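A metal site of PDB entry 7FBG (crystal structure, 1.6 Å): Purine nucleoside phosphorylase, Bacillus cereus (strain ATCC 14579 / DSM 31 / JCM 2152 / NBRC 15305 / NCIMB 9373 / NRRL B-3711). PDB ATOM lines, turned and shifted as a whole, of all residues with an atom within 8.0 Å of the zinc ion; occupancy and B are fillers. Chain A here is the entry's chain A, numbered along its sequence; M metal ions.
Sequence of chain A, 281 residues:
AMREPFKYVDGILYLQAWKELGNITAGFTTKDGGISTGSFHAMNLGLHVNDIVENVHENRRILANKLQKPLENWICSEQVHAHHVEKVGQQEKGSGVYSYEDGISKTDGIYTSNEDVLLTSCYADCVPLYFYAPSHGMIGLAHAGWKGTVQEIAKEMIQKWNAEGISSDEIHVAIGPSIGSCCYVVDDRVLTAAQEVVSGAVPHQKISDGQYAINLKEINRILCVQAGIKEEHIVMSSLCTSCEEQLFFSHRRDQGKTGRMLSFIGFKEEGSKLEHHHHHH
The side-chain sulfur (SG) of Cys 183 lies within hydrogen-bond range of the side-chain hydroxyl (OG) of Ser 242 (3.2 Å).
The side-chain sulfur of Cys 240 lies close to the backbone NH of Gly 180 (3.3 Å).
The side-chain sulfur (SG) of Cys 243 sits close to the side-chain sulfur (SG) of Cys 183 (3.7 Å).
SG of Cys 240 lies close to N of Ser 242 (3.4 Å).
The zinc ion is bound by SG of Cys 182 (2.0 Å), SG of Cys 243 (2.3 Å) and SG of Cys 240 (2.4 Å).
The zinc ion has three donor atoms within binding distance.
Slightly farther from the zinc ion lies the side-chain sulfur (SG) of Cys 183 (2.8 Å).
Four residues have an atom within 4 Å of the zinc ion: Cys 182, Cys 183, Cys 240 and Cys 243.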
ATOM      1  N   SER A 178      25.676 -14.172  -3.893  1.00  0.00           N
ATOM      2  CA  SER A 178      26.836 -14.156  -2.976  1.00  0.00           C
ATOM      3  C   SER A 178      26.300 -14.150  -1.554  1.00  0.00           C
ATOM      4  O   SER A 178      25.095 -14.065  -1.391  1.00  0.00           O
ATOM      5  CB  SER A 178      27.675 -12.916  -3.183  1.00  0.00           C
ATOM      6  OG  SER A 178      27.192 -11.832  -2.421  1.00  0.00           O
ATOM      7  N   ILE A 179      27.209 -14.243  -0.577  1.00  0.00           N
ATOM      8  CA  ILE A 179      26.762 -14.158   0.842  1.00  0.00           C
ATOM      9  C   ILE A 179      26.316 -12.725   1.129  1.00  0.00           C
ATOM     10  O   ILE A 179      27.026 -11.809   0.775  1.00  0.00           O
ATOM     11  CB  ILE A 179      27.828 -14.715   1.816  1.00  0.00           C
ATOM     12  CG1 ILE A 179      27.226 -14.960   3.199  1.00  0.00           C
ATOM     13  CG2 ILE A 179      29.087 -13.863   1.862  1.00  0.00           C
ATOM     14  CD1 ILE A 179      28.103 -15.756   4.110  1.00  0.00           C
ATOM     15  N   GLY A 180      25.119 -12.578   1.672  1.00  0.00           N
ATOM     16  CA  GLY A 180      24.571 -11.242   1.916  1.00  0.00           C
ATOM     17  C   GLY A 180      24.878 -10.751   3.310  1.00  0.00           C
ATOM     18  O   GLY A 180      25.443 -11.503   4.069  1.00  0.00           O
ATOM     19  N   SER A 181      24.463  -9.521   3.639  1.00  0.00           N
ATOM     20  CA  SER A 181      24.764  -8.884   4.945  1.00  0.00           C
ATOM     21  C   SER A 181      23.960  -9.601   6.025  1.00  0.00           C
ATOM     22  O   SER A 181      24.288  -9.464   7.184  1.00  0.00           O
ATOM     23  CB  SER A 181      24.404  -7.437   4.913  1.00  0.00           C
ATOM     24  OG  SER A 181      23.032  -7.257   4.597  1.00  0.00           O
ATOM     25  N   CYS A 182      22.929 -10.302   5.612  1.00  0.00           N
ATOM     26  CA  CYS A 182      22.133 -11.109   6.562  1.00  0.00           C
ATOM     27  C   CYS A 182      22.998 -12.183   7.195  1.00  0.00           C
ATOM     28  O   CYS A 182      22.730 -12.558   8.334  1.00  0.00           O
ATOM     29  CB  CYS A 182      21.030 -11.796   5.783  1.00  0.00           C
ATOM     30  SG  CYS A 182      21.577 -12.309   4.133  1.00  0.00           S
ATOM     31  N   CYS A 183      24.035 -12.641   6.483  1.00  0.00           N
ATOM     32  CA  CYS A 183      24.831 -13.788   6.977  1.00  0.00           C
ATOM     33  C   CYS A 183      26.326 -13.492   7.043  1.00  0.00           C
ATOM     34  O   CYS A 183      27.035 -14.293   7.614  1.00  0.00           O
ATOM     35  CB  CYS A 183      24.723 -14.959   6.015  1.00  0.00           C
ATOM     36  SG  CYS A 183      23.032 -15.614   5.968  1.00  0.00           S
ATOM     37  N   TYR A 184      26.755 -12.389   6.456  1.00  0.00           N
ATOM     38  CA  TYR A 184      28.218 -12.147   6.384  1.00  0.00           C
ATOM     39  C   TYR A 184      28.631 -11.065   7.387  1.00  0.00           C
ATOM     40  O   TYR A 184      28.356  -9.893   7.161  1.00  0.00           O
ATOM     41  CB  TYR A 184      28.634 -11.774   4.967  1.00  0.00           C
ATOM     42  CG  TYR A 184      30.118 -11.756   4.712  1.00  0.00           C
ATOM     43  CD1 TYR A 184      30.949 -12.766   5.180  1.00  0.00           C
ATOM     44  CD2 TYR A 184      30.693 -10.733   3.988  1.00  0.00           C
ATOM     45  CE1 TYR A 184      32.308 -12.738   4.934  1.00  0.00           C
ATOM     46  CE2 TYR A 184      32.048 -10.697   3.740  1.00  0.00           C
ATOM     47  CZ  TYR A 184      32.857 -11.705   4.209  1.00  0.00           C
ATOM     48  OH  TYR A 184      34.194 -11.656   3.959  1.00  0.00           O
ATOM     49  N   LYS A 217      28.209  -7.247  -2.313  1.00  0.00           N
ATOM     50  CA  LYS A 217      27.644  -6.946  -3.664  1.00  0.00           C
ATOM     51  C   LYS A 217      27.576  -5.424  -3.833  1.00  0.00           C
ATOM     52  O   LYS A 217      28.007  -4.928  -4.868  1.00  0.00           O
ATOM     53  CB  LYS A 217      26.223  -7.482  -3.818  1.00  0.00           C
ATOM     54  CG  LYS A 217      26.060  -8.991  -3.937  1.00  0.00           C
ATOM     55  CD  LYS A 217      24.599  -9.344  -4.062  1.00  0.00           C
ATOM     56  CE  LYS A 217      24.300 -10.822  -3.946  1.00  0.00           C
ATOM     57  NZ  LYS A 217      24.272 -11.266  -2.533  1.00  0.00           N
ATOM     58  N   SER A 238      20.035 -10.060  -5.500  1.00  0.00           N
ATOM     59  CA  SER A 238      19.905  -9.885  -4.035  1.00  0.00           C
ATOM     60  C   SER A 238      19.976 -11.266  -3.363  1.00  0.00           C
ATOM     61  O   SER A 238      19.818 -11.349  -2.160  1.00  0.00           O
ATOM     62  CB  SER A 238      18.588  -9.242  -3.693  1.00  0.00           C
ATOM     63  OG  SER A 238      17.511 -10.010  -4.185  1.00  0.00           O
ATOM     64  N   LEU A 239      20.214 -12.298  -4.160  1.00  0.00           N
ATOM     65  CA  LEU A 239      20.198 -13.679  -3.618  1.00  0.00           C
ATOM     66  C   LEU A 239      21.389 -13.911  -2.697  1.00  0.00           C
ATOM     67  O   LEU A 239      22.492 -13.493  -3.024  1.00  0.00           O
ATOM     68  CB  LEU A 239      20.180 -14.692  -4.756  1.00  0.00           C
ATOM     69  CG  LEU A 239      18.863 -14.803  -5.521  1.00  0.00           C
ATOM     70  CD1 LEU A 239      19.048 -15.632  -6.780  1.00  0.00           C
ATOM     71  CD2 LEU A 239      17.782 -15.404  -4.642  1.00  0.00           C
ATOM     72  N   CYS A 240      21.125 -14.588  -1.577  1.00  0.00           N
ATOM     73  CA  CYS A 240      22.183 -14.897  -0.608  1.00  0.00           C
ATOM     74  C   CYS A 240      22.481 -16.395  -0.649  1.00  0.00           C
ATOM     75  O   CYS A 240      21.566 -17.178  -0.487  1.00  0.00           O
ATOM     76  CB  CYS A 240      21.751 -14.517   0.809  1.00  0.00           C
ATOM     77  SG  CYS A 240      22.935 -15.088   2.061  1.00  0.00           S
ATOM     78  N   THR A 241      23.744 -16.737  -0.851  1.00  0.00           N
ATOM     79  CA  THR A 241      24.157 -18.151  -0.961  1.00  0.00           C
ATOM     80  C   THR A 241      23.886 -18.921   0.338  1.00  0.00           C
ATOM     81  O   THR A 241      23.592 -20.103   0.263  1.00  0.00           O
ATOM     82  CB  THR A 241      25.645 -18.189  -1.346  1.00  0.00           C
ATOM     83  OG1 THR A 241      26.320 -17.247  -0.534  1.00  0.00           O
ATOM     84  CG2 THR A 241      25.848 -17.891  -2.813  1.00  0.00           C
ATOM     85  N   SER A 242      24.065 -18.256   1.467  1.00  0.00           N
ATOM     86  CA  SER A 242      23.879 -18.936   2.770  1.00  0.00           C
ATOM     87  C   SER A 242      22.396 -19.139   3.064  1.00  0.00           C
ATOM     88  O   SER A 242      22.030 -20.198   3.526  1.00  0.00           O
ATOM     89  CB  SER A 242      24.576 -18.151   3.853  1.00  0.00           C
ATOM     90  OG  SER A 242      24.094 -18.526   5.129  1.00  0.00           O
ATOM     91  N   CYS A 243      21.569 -18.151   2.761  1.00  0.00           N
ATOM     92  CA  CYS A 243      20.128 -18.253   3.092  1.00  0.00           C
ATOM     93  C   CYS A 243      19.455 -19.280   2.180  1.00  0.00           C
ATOM     94  O   CYS A 243      18.508 -19.929   2.640  1.00  0.00           O
ATOM     95  CB  CYS A 243      19.435 -16.908   2.882  1.00  0.00           C
ATOM     96  SG  CYS A 243      19.769 -15.717   4.217  1.00  0.00           S
ATOM     97  N   GLU A 244      19.876 -19.347   0.916  1.00  0.00           N
ATOM     98  CA  GLU A 244      19.164 -20.234  -0.048  1.00  0.00           C
ATOM     99  C   GLU A 244      19.756 -21.637   0.053  1.00  0.00           C
ATOM    100  O   GLU A 244      20.516 -22.016  -0.827  1.00  0.00           O
ATOM    101  CB  GLU A 244      19.198 -19.647  -1.455  1.00  0.00           C
ATOM    102  CG  GLU A 244      18.669 -18.235  -1.554  1.00  0.00           C
ATOM    103  CD  GLU A 244      17.173 -18.039  -1.336  1.00  0.00           C
ATOM    104  OE1 GLU A 244      16.446 -19.036  -1.291  1.00  0.00           O
ATOM    105  OE2 GLU A 244      16.758 -16.883  -1.236  1.00  0.00           O
HETATM  106 ZN    ZN M   1      21.577 -14.292   3.919  1.00  0.00          ZN
